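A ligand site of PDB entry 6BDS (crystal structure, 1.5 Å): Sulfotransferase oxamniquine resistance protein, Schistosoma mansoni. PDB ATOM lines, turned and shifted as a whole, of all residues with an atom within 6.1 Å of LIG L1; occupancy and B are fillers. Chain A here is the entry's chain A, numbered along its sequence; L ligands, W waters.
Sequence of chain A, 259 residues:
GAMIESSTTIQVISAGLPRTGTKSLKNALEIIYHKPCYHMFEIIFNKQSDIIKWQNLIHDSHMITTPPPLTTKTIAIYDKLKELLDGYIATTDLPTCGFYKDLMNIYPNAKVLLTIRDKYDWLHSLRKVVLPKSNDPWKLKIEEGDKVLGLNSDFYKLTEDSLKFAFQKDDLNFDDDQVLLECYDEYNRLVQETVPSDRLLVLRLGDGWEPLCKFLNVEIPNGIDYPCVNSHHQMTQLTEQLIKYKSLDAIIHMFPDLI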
ATOM      1  N   LEU A  17      12.822 -18.836  10.658  1.00  0.00           N
ATOM      2  CA  LEU A  17      11.979 -17.646  10.803  1.00  0.00           C
ATOM      3  C   LEU A  17      12.751 -16.500  11.447  1.00  0.00           C
ATOM      4  O   LEU A  17      13.792 -16.696  12.075  1.00  0.00           O
ATOM      5  CB  LEU A  17      10.748 -17.978  11.641  1.00  0.00           C
ATOM      6  CG  LEU A  17       9.760 -18.935  10.977  1.00  0.00           C
ATOM      7  CD1 LEU A  17       8.812 -19.542  11.993  1.00  0.00           C
ATOM      8  CD2 LEU A  17       8.971 -18.231   9.865  1.00  0.00           C
ATOM      9  N   PRO A  18      12.256 -15.277  11.327  1.00  0.00           N
ATOM     10  CA  PRO A  18      12.896 -14.172  12.025  1.00  0.00           C
ATOM     11  C   PRO A  18      12.971 -14.453  13.522  1.00  0.00           C
ATOM     12  O   PRO A  18      12.116 -15.122  14.091  1.00  0.00           O
ATOM     13  CB  PRO A  18      11.994 -12.974  11.693  1.00  0.00           C
ATOM     14  CG  PRO A  18      10.738 -13.573  11.214  1.00  0.00           C
ATOM     15  CD  PRO A  18      11.091 -14.834  10.551  1.00  0.00           C
ATOM     16  N   ARG A  19      14.053 -13.955  14.127  1.00  0.00           N
ATOM     17  CA  ARG A  19      14.330 -14.055  15.563  1.00  0.00           C
ATOM     18  C   ARG A  19      14.741 -15.463  15.982  1.00  0.00           C
ATOM     19  O   ARG A  19      14.590 -15.848  17.157  1.00  0.00           O
ATOM     20  CB  ARG A  19      13.143 -13.563  16.414  1.00  0.00           C
ATOM     21  CG  ARG A  19      12.642 -12.184  16.035  1.00  0.00           C
ATOM     22  CD  ARG A  19      13.761 -11.111  15.946  1.00  0.00           C
ATOM     23  NE  ARG A  19      14.451 -10.882  17.206  1.00  0.00           N
ATOM     24  CZ  ARG A  19      15.555 -10.151  17.379  1.00  0.00           C
ATOM     25  NH1 ARG A  19      16.148  -9.571  16.358  1.00  0.00           N
ATOM     26  NH2 ARG A  19      16.070 -10.006  18.582  1.00  0.00           N
ATOM     27  N   THR A  20      15.310 -16.233  15.041  1.00  0.00           N
ATOM     28  CA  THR A  20      15.878 -17.553  15.333  1.00  0.00           C
ATOM     29  C   THR A  20      17.385 -17.614  15.084  1.00  0.00           C
ATOM     30  O   THR A  20      17.931 -18.710  14.921  1.00  0.00           O
ATOM     31  CB  THR A  20      15.186 -18.656  14.519  1.00  0.00           C
ATOM     32  OG1 THR A  20      15.396 -18.453  13.110  1.00  0.00           O
ATOM     33  CG2 THR A  20      13.726 -18.707  14.798  1.00  0.00           C
ATOM     34  N   GLY A  21      18.071 -16.479  15.066  1.00  0.00           N
ATOM     35  CA  GLY A  21      19.499 -16.419  14.770  1.00  0.00           C
ATOM     36  C   GLY A  21      19.846 -16.116  13.332  1.00  0.00           C
ATOM     37  O   GLY A  21      20.960 -16.456  12.887  1.00  0.00           O
ATOM     38  N   THR A  22      18.943 -15.490  12.582  1.00  0.00           N
ATOM     39  CA  THR A  22      19.177 -15.253  11.158  1.00  0.00           C
ATOM     40  C   THR A  22      20.330 -14.276  10.920  1.00  0.00           C
ATOM     41  O   THR A  22      21.082 -14.423   9.952  1.00  0.00           O
ATOM     42  CB  THR A  22      17.925 -14.726  10.458  1.00  0.00           C
ATOM     43  OG1 THR A  22      17.582 -13.414  10.926  1.00  0.00           O
ATOM     44  CG2 THR A  22      16.752 -15.660  10.656  1.00  0.00           C
ATOM     45  N   LYS A  23      20.448 -13.240  11.751  1.00  0.00           N
ATOM     46  CA  LYS A  23      21.490 -12.251  11.487  1.00  0.00           C
ATOM     47  C   LYS A  23      22.864 -12.827  11.826  1.00  0.00           C
ATOM     48  O   LYS A  23      23.837 -12.599  11.105  1.00  0.00           O
ATOM     49  CB  LYS A  23      21.218 -10.962  12.272  1.00  0.00           C
ATOM     50  CG  LYS A  23      22.220  -9.835  12.004  1.00  0.00           C
ATOM     51  CD  LYS A  23      22.328  -9.531  10.507  1.00  0.00           C
ATOM     52  CE  LYS A  23      23.002  -8.201  10.206  1.00  0.00           C
ATOM     53  NZ  LYS A  23      24.450  -8.177  10.495  1.00  0.00           N
ATOM     54  N   SER A  24      22.942 -13.617  12.895  1.00  0.00           N
ATOM     55  CA  SER A  24      24.194 -14.298  13.186  1.00  0.00           C
ATOM     56  C   SER A  24      24.571 -15.247  12.064  1.00  0.00           C
ATOM     57  O   SER A  24      25.749 -15.355  11.692  1.00  0.00           O
ATOM     58  CB  SER A  24      24.094 -15.065  14.509  1.00  0.00           C
ATOM     59  OG  SER A  24      24.039 -14.178  15.605  1.00  0.00           O
ATOM     60  N   HIS A  39      19.028 -10.915   3.794  1.00  0.00           N
ATOM     61  CA  HIS A  39      18.471 -10.773   5.131  1.00  0.00           C
ATOM     62  C   HIS A  39      17.565  -9.551   5.081  1.00  0.00           C
ATOM     63  O   HIS A  39      17.704  -8.714   4.195  1.00  0.00           O
ATOM     64  CB  HIS A  39      19.600 -10.599   6.150  1.00  0.00           C
ATOM     65  CG  HIS A  39      19.151 -10.616   7.573  1.00  0.00           C
ATOM     66  ND1 HIS A  39      18.748  -9.472   8.249  1.00  0.00           N
ATOM     67  CD2 HIS A  39      19.083 -11.630   8.473  1.00  0.00           C
ATOM     68  CE1 HIS A  39      18.434  -9.804   9.492  1.00  0.00           C
ATOM     69  NE2 HIS A  39      18.618 -11.097   9.647  1.00  0.00           N
ATOM     70  N   ASP A  93      16.052 -15.162   6.562  1.00  0.00           N
ATOM     71  CA  ASP A  93      15.127 -14.173   7.114  1.00  0.00           C
ATOM     72  C   ASP A  93      13.940 -13.936   6.194  1.00  0.00           C
ATOM     73  O   ASP A  93      13.915 -14.399   5.060  1.00  0.00           O
ATOM     74  CB  ASP A  93      15.876 -12.869   7.349  1.00  0.00           C
ATOM     75  CG  ASP A  93      15.194 -11.932   8.333  1.00  0.00           C
ATOM     76  OD1 ASP A  93      14.200 -12.315   8.999  1.00  0.00           O
ATOM     77  OD2 ASP A  93      15.699 -10.788   8.442  1.00  0.00           O
ATOM     78  N   ARG A 117      14.362 -22.498  17.784  1.00  0.00           N
ATOM     79  CA  ARG A 117      14.599 -22.214  19.187  1.00  0.00           C
ATOM     80  C   ARG A 117      13.290 -22.426  19.936  1.00  0.00           C
ATOM     81  O   ARG A 117      12.225 -22.680  19.343  1.00  0.00           O
ATOM     82  CB  ARG A 117      15.112 -20.779  19.397  1.00  0.00           C
ATOM     83  CG  ARG A 117      14.007 -19.743  19.166  1.00  0.00           C
ATOM     84  CD  ARG A 117      14.500 -18.334  19.173  1.00  0.00           C
ATOM     85  NE  ARG A 117      15.002 -17.904  20.469  1.00  0.00           N
ATOM     86  CZ  ARG A 117      15.358 -16.660  20.764  1.00  0.00           C
ATOM     87  NH1 ARG A 117      15.211 -15.674  19.879  1.00  0.00           N
ATOM     88  NH2 ARG A 117      15.849 -16.398  21.979  1.00  0.00           N
ATOM     89  N   ASP A 121      10.576 -18.231  23.784  1.00  0.00           N
ATOM     90  CA  ASP A 121      11.684 -17.293  23.583  1.00  0.00           C
ATOM     91  C   ASP A 121      11.553 -16.586  22.248  1.00  0.00           C
ATOM     92  O   ASP A 121      11.823 -15.382  22.138  1.00  0.00           O
ATOM     93  CB  ASP A 121      13.033 -18.025  23.605  1.00  0.00           C
ATOM     94  CG  ASP A 121      13.438 -18.546  25.002  1.00  0.00           C
ATOM     95  OD1 ASP A 121      12.816 -18.154  26.030  1.00  0.00           O
ATOM     96  OD2 ASP A 121      14.400 -19.361  25.064  1.00  0.00           O
ATOM     97  N   HIS A 124       8.655 -13.973  22.447  1.00  0.00           N
ATOM     98  CA  HIS A 124       9.083 -12.852  23.214  1.00  0.00           C
ATOM     99  C   HIS A 124       9.993 -11.942  22.411  1.00  0.00           C
ATOM    100  O   HIS A 124       9.823 -10.782  22.421  1.00  0.00           O
ATOM    101  CB  HIS A 124       9.754 -13.379  24.509  1.00  0.00           C
ATOM    102  CG  HIS A 124      10.360 -12.327  25.372  1.00  0.00           C
ATOM    103  ND1 HIS A 124       9.619 -11.496  26.168  1.00  0.00           N
ATOM    104  CD2 HIS A 124      11.650 -11.994  25.585  1.00  0.00           C
ATOM    105  CE1 HIS A 124      10.428 -10.685  26.814  1.00  0.00           C
ATOM    106  NE2 HIS A 124      11.655 -10.973  26.491  1.00  0.00           N
ATOM    107  N   SER A 125      10.940 -12.545  21.729  1.00  0.00           N
ATOM    108  CA  SER A 125      11.840 -11.790  20.864  1.00  0.00           C
ATOM    109  C   SER A 125      11.068 -11.091  19.753  1.00  0.00           C
ATOM    110  O   SER A 125      11.284  -9.899  19.479  1.00  0.00           O
ATOM    111  CB  SER A 125      12.872 -12.754  20.286  1.00  0.00           C
ATOM    112  OG  SER A 125      13.914 -12.068  19.630  1.00  0.00           O
ATOM    113  N   VAL A 129      10.798  -6.845  18.957  1.00  0.00           N
ATOM    114  CA  VAL A 129      11.585  -6.324  17.834  1.00  0.00           C
ATOM    115  C   VAL A 129      10.731  -6.135  16.575  1.00  0.00           C
ATOM    116  O   VAL A 129      10.856  -5.111  15.904  1.00  0.00           O
ATOM    117  CB  VAL A 129      12.781  -7.255  17.523  1.00  0.00           C
ATOM    118  CG1 VAL A 129      13.576  -6.780  16.311  1.00  0.00           C
ATOM    119  CG2 VAL A 129      13.679  -7.336  18.726  1.00  0.00           C
ATOM    120  N   LEU A 205      20.043 -22.363  18.325  1.00  0.00           N
ATOM    121  CA  LEU A 205      20.883 -21.310  18.857  1.00  0.00           C
ATOM    122  C   LEU A 205      21.904 -21.925  19.802  1.00  0.00           C
ATOM    123  O   LEU A 205      21.557 -22.735  20.657  1.00  0.00           O
ATOM    124  CB  LEU A 205      20.044 -20.266  19.586  1.00  0.00           C
ATOM    125  CG  LEU A 205      19.116 -19.390  18.770  1.00  0.00           C
ATOM    126  CD1 LEU A 205      18.359 -18.486  19.717  1.00  0.00           C
ATOM    127  CD2 LEU A 205      19.898 -18.580  17.741  1.00  0.00           C
ATOM    128  N   GLY A 206      23.178 -21.542  19.636  1.00  0.00           N
ATOM    129  CA  GLY A 206      24.269 -22.103  20.424  1.00  0.00           C
ATOM    130  C   GLY A 206      25.120 -23.128  19.701  1.00  0.00           C
ATOM    131  O   GLY A 206      26.247 -23.392  20.146  1.00  0.00           O
ATOM    132  N   TYR A 226      31.804 -17.863  16.510  1.00  0.00           N
ATOM    133  CA  TYR A 226      30.547 -17.847  15.793  1.00  0.00           C
ATOM    134  C   TYR A 226      29.771 -16.591  16.199  1.00  0.00           C
ATOM    135  O   TYR A 226      29.720 -16.260  17.388  1.00  0.00           O
ATOM    136  CB  TYR A 226      29.728 -19.101  16.076  1.00  0.00           C
ATOM    137  CG  TYR A 226      28.503 -19.179  15.225  1.00  0.00           C
ATOM    138  CD1 TYR A 226      28.527 -19.760  13.958  1.00  0.00           C
ATOM    139  CD2 TYR A 226      27.314 -18.639  15.661  1.00  0.00           C
ATOM    140  CE1 TYR A 226      27.389 -19.803  13.165  1.00  0.00           C
ATOM    141  CE2 TYR A 226      26.171 -18.658  14.887  1.00  0.00           C
ATOM    142  CZ  TYR A 226      26.214 -19.248  13.643  1.00  0.00           C
ATOM    143  OH  TYR A 226      25.070 -19.266  12.883  1.00  0.00           O
ATOM    144  N   PRO A 227      29.195 -15.853  15.249  1.00  0.00           N
ATOM    145  CA  PRO A 227      28.527 -14.593  15.602  1.00  0.00           C
ATOM    146  C   PRO A 227      27.435 -14.774  16.642  1.00  0.00           C
ATOM    147  O   PRO A 227      26.720 -15.771  16.664  1.00  0.00           O
ATOM    148  CB  PRO A 227      27.937 -14.123  14.279  1.00  0.00           C
ATOM    149  CG  PRO A 227      28.818 -14.710  13.260  1.00  0.00           C
ATOM    150  CD  PRO A 227      29.219 -16.054  13.781  1.00  0.00           C
ATOM    151  N   CYS A 228      27.271 -13.746  17.470  1.00  0.00           N
ATOM    152  CA  CYS A 228      26.207 -13.698  18.467  1.00  0.00           C
ATOM    153  C   CYS A 228      25.721 -12.252  18.482  1.00  0.00           C
ATOM    154  O   CYS A 228      26.190 -11.418  19.255  1.00  0.00           O
ATOM    155  CB  CYS A 228      26.708 -14.133  19.834  1.00  0.00           C
ATOM    156  SG  CYS A 228      25.403 -14.262  21.060  1.00  0.00           S
ATOM    157  N   VAL A 229      24.852 -11.939  17.541  1.00  0.00           N
ATOM    158  CA  VAL A 229      24.362 -10.589  17.413  1.00  0.00           C
ATOM    159  C   VAL A 229      22.852 -10.593  17.368  1.00  0.00           C
ATOM    160  O   VAL A 229      22.242 -11.644  17.483  1.00  0.00           O
ATOM    161  CB  VAL A 229      24.883  -9.966  16.103  1.00  0.00           C
ATOM    162  CG1 VAL A 229      26.379  -9.776  16.163  1.00  0.00           C
ATOM    163  CG2 VAL A 229      24.508 -10.847  14.918  1.00  0.00           C
ATOM    164  N   ASN A 230      22.313  -9.377  17.254  1.00  0.00           N
ATOM    165  CA  ASN A 230      20.891  -9.101  17.117  1.00  0.00           C
ATOM    166  C   ASN A 230      19.964  -9.450  18.273  1.00  0.00           C
ATOM    167  O   ASN A 230      18.815  -9.739  18.055  1.00  0.00           O
ATOM    168  CB  ASN A 230      20.354  -9.717  15.802  1.00  0.00           C
ATOM    169  CG  ASN A 230      19.687  -8.723  14.918  1.00  0.00           C
ATOM    170  OD1 ASN A 230      20.145  -7.603  14.771  1.00  0.00           O
ATOM    171  ND2 ASN A 230      18.620  -9.159  14.280  1.00  0.00           N
ATOM    172  N   SER A 231      20.455  -9.372  19.507  1.00  0.00           N
ATOM    173  CA  SER A 231      19.610  -9.632  20.668  1.00  0.00           C
ATOM    174  C   SER A 231      18.530  -8.559  20.804  1.00  0.00           C
ATOM    175  O   SER A 231      18.743  -7.415  20.419  1.00  0.00           O
ATOM    176  CB  SER A 231      20.438  -9.686  21.952  1.00  0.00           C
ATOM    177  OG  SER A 231      20.897  -8.394  22.319  1.00  0.00           O
ATOM    178  N   HIS A 232      17.387  -8.894  21.370  1.00  0.00           N
ATOM    179  CA  HIS A 232      16.360  -7.874  21.469  1.00  0.00           C
ATOM    180  C   HIS A 232      16.828  -6.722  22.342  1.00  0.00           C
ATOM    181  O   HIS A 232      16.451  -5.573  22.096  1.00  0.00           O
ATOM    182  CB  HIS A 232      15.027  -8.458  21.951  1.00  0.00           C
ATOM    183  CG  HIS A 232      15.003  -8.892  23.382  1.00  0.00           C
ATOM    184  ND1 HIS A 232      14.871  -8.004  24.440  1.00  0.00           N
ATOM    185  CD2 HIS A 232      15.023 -10.128  23.938  1.00  0.00           C
ATOM    186  CE1 HIS A 232      14.857  -8.688  25.575  1.00  0.00           C
ATOM    187  NE2 HIS A 232      14.940  -9.983  25.294  1.00  0.00           N
ATOM    188  N   HIS A 233      17.699  -7.004  23.316  1.00  0.00           N
ATOM    189  CA  HIS A 233      18.237  -5.929  24.125  1.00  0.00           C
ATOM    190  C   HIS A 233      19.004  -4.946  23.262  1.00  0.00           C
ATOM    191  O   HIS A 233      18.919  -3.731  23.464  1.00  0.00           O
ATOM    192  CB  HIS A 233      19.158  -6.492  25.212  1.00  0.00           C
ATOM    193  CG  HIS A 233      18.431  -7.276  26.256  1.00  0.00           C
ATOM    194  ND1 HIS A 233      17.646  -6.685  27.215  1.00  0.00           N
ATOM    195  CD2 HIS A 233      18.361  -8.613  26.474  1.00  0.00           C
ATOM    196  CE1 HIS A 233      17.130  -7.621  27.992  1.00  0.00           C
ATOM    197  NE2 HIS A 233      17.557  -8.794  27.575  1.00  0.00           N
HETATM  198  P1  LIG L   1      16.842 -12.629  21.675  1.00  0.00           P
HETATM  199  O1  LIG L   1      16.051 -13.597  22.508  1.00  0.00           O
HETATM  200  O2  LIG L   1      15.975 -11.565  21.047  1.00  0.00           O
HETATM  201  O3  LIG L   1      18.097 -12.076  22.334  1.00  0.00           O
HETATM  202  P2  LIG L   1      17.506 -12.854  14.369  1.00  0.00           P
HETATM  203  O4  LIG L   1      16.918 -13.964  13.496  1.00  0.00           O
HETATM  204  O5  LIG L   1      18.933 -12.460  14.038  1.00  0.00           O
HETATM  205  O6  LIG L   1      16.574 -11.678  14.512  1.00  0.00           O
HETATM  206  O7  LIG L   1      17.599 -13.643  15.799  1.00  0.00           O
HETATM  207  C1  LIG L   1      18.092 -12.953  16.923  1.00  0.00           C
HETATM  208  C2  LIG L   1      17.938 -13.848  18.159  1.00  0.00           C
HETATM  209  O8  LIG L   1      18.911 -14.928  18.154  1.00  0.00           O
HETATM  210  C3  LIG L   1      18.177 -13.085  19.452  1.00  0.00           C
HETATM  211  O9  LIG L   1      17.337 -13.585  20.473  1.00  0.00           O
HETATM  212  C4  LIG L   1      19.644 -13.371  19.691  1.00  0.00           C
HETATM  213  O10 LIG L   1      20.019 -13.087  21.035  1.00  0.00           O
HETATM  214  C5  LIG L   1      19.735 -14.828  19.321  1.00  0.00           C
HETATM  215  N1  LIG L   1      21.089 -15.271  18.971  1.00  0.00           N
HETATM  216  C6  LIG L   1      21.765 -14.885  17.866  1.00  0.00           C
HETATM  217  N2  LIG L   1      22.978 -15.486  17.811  1.00  0.00           N
HETATM  218  C7  LIG L   1      23.071 -16.262  18.907  1.00  0.00           C
HETATM  219  C8  LIG L   1      24.090 -17.146  19.472  1.00  0.00           C
HETATM  220  N3  LIG L   1      25.228 -17.304  18.797  1.00  0.00           N
HETATM  221  N4  LIG L   1      23.806 -17.803  20.610  1.00  0.00           N
HETATM  222  C9  LIG L   1      22.636 -17.619  21.254  1.00  0.00           C
HETATM  223  N5  LIG L   1      21.655 -16.801  20.808  1.00  0.00           N
HETATM  224  C10 LIG L   1      21.833 -16.119  19.665  1.00  0.00           C
HETATM  225  C1  LG2 L   2      11.787  -8.004  10.157  1.00  0.00           C
HETATM  226  C2  LG2 L   2      12.925  -8.296  10.880  1.00  0.00           C
HETATM  227  C3  LG2 L   2      12.701  -6.216  12.141  1.00  0.00           C
HETATM  228  C4  LG2 L   2      11.132  -6.812  10.430  1.00  0.00           C
HETATM  229  C5  LG2 L   2      13.587  -9.598  10.515  1.00  0.00           C
HETATM  230  N1  LG2 L   2      14.517  -7.711  12.678  1.00  0.00           N
HETATM  231  C6  LG2 L   2      14.473  -2.174  13.977  1.00  0.00           C
HETATM  232  C7  LG2 L   2      16.905  -2.115  12.629  1.00  0.00           C
HETATM  233  C8  LG2 L   2      15.054  -0.953  13.637  1.00  0.00           C
HETATM  234  C9  LG2 L   2      16.264  -0.924  12.959  1.00  0.00           C
HETATM  235  C10 LG2 L   2      10.910  -3.465  12.041  1.00  0.00           C
HETATM  236  C11 LG2 L   2       9.964  -3.223  13.215  1.00  0.00           C
HETATM  237  C12 LG2 L   2      10.815  -2.495  14.244  1.00  0.00           C
HETATM  238  C13 LG2 L   2      16.320  -3.331  12.947  1.00  0.00           C
HETATM  239  C14 LG2 L   2      12.284  -2.975  12.489  1.00  0.00           C
HETATM  240  C15 LG2 L   2      15.123  -3.360  13.632  1.00  0.00           C
HETATM  241  C16 LG2 L   2      18.200  -2.135  11.873  1.00  0.00           C
HETATM  242  C17 LG2 L   2      13.381  -7.424  11.884  1.00  0.00           C
HETATM  243  C18 LG2 L   2      11.568  -5.915  11.396  1.00  0.00           C
HETATM  244  C19 LG2 L   2      13.137  -2.234  14.687  1.00  0.00           C
HETATM  245  F1  LG2 L   2      18.021  -2.809  10.754  1.00  0.00           F
HETATM  246  F2  LG2 L   2      18.563  -0.906  11.559  1.00  0.00           F
HETATM  247  F3  LG2 L   2      19.154  -2.746  12.553  1.00  0.00           F
HETATM  248  N2  LG2 L   2      10.777  -4.827  11.550  1.00  0.00           N
HETATM  249  N3  LG2 L   2      12.088  -2.082  13.650  1.00  0.00           N
HETATM  250  O1  LG2 L   2      14.670  -8.842  13.197  1.00  0.00           O
HETATM  251  O2  LG2 L   2      15.359  -6.848  12.946  1.00  0.00           O
HETATM  252  O3  LG2 L   2      15.037  -9.481  10.458  1.00  0.00           O
HETATM  253  O   HOH W   1      17.062 -14.263  24.981  1.00  0.00           O
HETATM  254  O   HOH W   2      16.998 -10.038  12.337  1.00  0.00           O
HETATM  255  O   HOH W   3      18.720 -11.676  24.814  1.00  0.00           O
HETATM  256  O   HOH W   4      25.580 -19.048  22.143  1.00  0.00           O
HETATM  257  O   HOH W   5      19.715 -16.920  23.073  1.00  0.00           O
HETATM  258  O   HOH W   6      13.669 -14.021  23.832  1.00  0.00           O
HETATM  259  O   HOH W   7      21.169 -13.293  15.137  1.00  0.00           O
HETATM  260  O   HOH W   8      27.365 -19.697  19.092  1.00  0.00           O
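The side-chain hydroxyl of Ser 125 sits at hydrogen-bond distance from the guanidinium group of Arg 19 (2.8 Å).
The side-chain hydroxyl of Ser 24 sits at hydrogen-bond distance from the backbone carbonyl oxygen of Pro 227, at 3.3 Å.
The guanidinium group of Arg 19 lies within hydrogen-bond range of the backbone carbonyl oxygen of Asn 230.
OG of Ser 24 sits at hydrogen-bond distance from N of Val 229.
OG1 of Thr 20 lies within hydrogen-bond range of O of Leu 17, 2.6 Å away.
The side-chain hydroxyl of Thr 22 lies within hydrogen-bond range of a ring nitrogen (NE2) of His 39 (2.8 Å).
The backbone carbonyl oxygen of Arg 19 sits at hydrogen-bond distance from the guanidinium group of Arg 117.
N of Lys 23 is in hydrogen-bond range of O5 of LIG L1 (2.9 Å).
The backbone carbonyl oxygen (O) of Pro 227 sits at hydrogen-bond distance from a nitrogen (N3) of LIG L1 (3.0 Å).
The backbone NH (N) of Gly 21 lies within hydrogen-bond range of an oxygen (O7) of LIG L1, 3.0 Å away.
The backbone NH (N) of Thr 22 lies within hydrogen-bond range of an oxygen (O4) of LIG L1, 2.7 Å away.
OG of Ser 125 sits at hydrogen-bond distance from O2 of LIG L1 (2.6 Å).
N of Arg 19 is in hydrogen-bond range of O4 of LIG L1 (2.9 Å).
OG of Ser 24 sits at hydrogen-bond distance from N2 of LIG L1 (2.8 Å).
The side-chain sulfur of Cys 228 sits close to a nitrogen (N3) of LIG L1, at 3.8 Å.
OG1 of Thr 22 sits at hydrogen-bond distance from O4 of LIG L1, 2.7 Å away.
N of His 232 is in hydrogen-bond range of O2 of LIG L1, 3.0 Å away.
NH1 of Arg 19 lies within salt-bridge range of O6 of LIG L1, 2.8 Å away.
An oxygen (O6) of LIG L1 lies within hydrogen-bond range of the side-chain amide nitrogen of Asn 230 (3.3 Å).
OD2 of Asp 93 lies within hydrogen-bond range of O3 of LG2 L2 (2.5 Å).
The backbone NH (N) of Thr 20 is in hydrogen-bond range of an oxygen (O4) of LIG L1, 3.2 Å away.
The guanidinium group (NH2) of Arg 117 lies within salt-bridge range of an oxygen (O1) of LIG L1.
Pro 18 touches LIG L1.
CD2 of Leu 205 touches C10 of LIG L1 (3.7 Å).
N of Gly 206 touches N4 of LIG L1, 3.9 Å away.
Tyr 226 touches LIG L1 (CD2 to N3, 3.996 Å).
O of Val 229 touches C6 of LIG L1, 3.3 Å away.
Ser 231 touches LIG L1.
Hydrophobic or aromatic side chains within 4 Å of LIG L1: Leu 205, Tyr 226 and His 232.
The nearest printed residue that does not touch LIG L1 is Leu 17 (4.4 Å).
Water W7 lies within hydrogen-bond range of O5 of LIG L1 (2.6 Å), N of Ser 24 (2.9 Å), O of Val 229 (3.1 Å) and N of Lys 23 (3.5 Å).
Water W2 lies within hydrogen-bond range of ND2 of Asn 230 (2.7 Å), O1 of LG2 L2 (2.8 Å), O6 of LIG L1 (2.8 Å) and NE2 of His 39 (3.3 Å).
Water W6 bridges an oxygen (O1) of LIG L1 (2.8 Å) and the backbone carbonyl oxygen of Asp 121 (2.9 Å).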
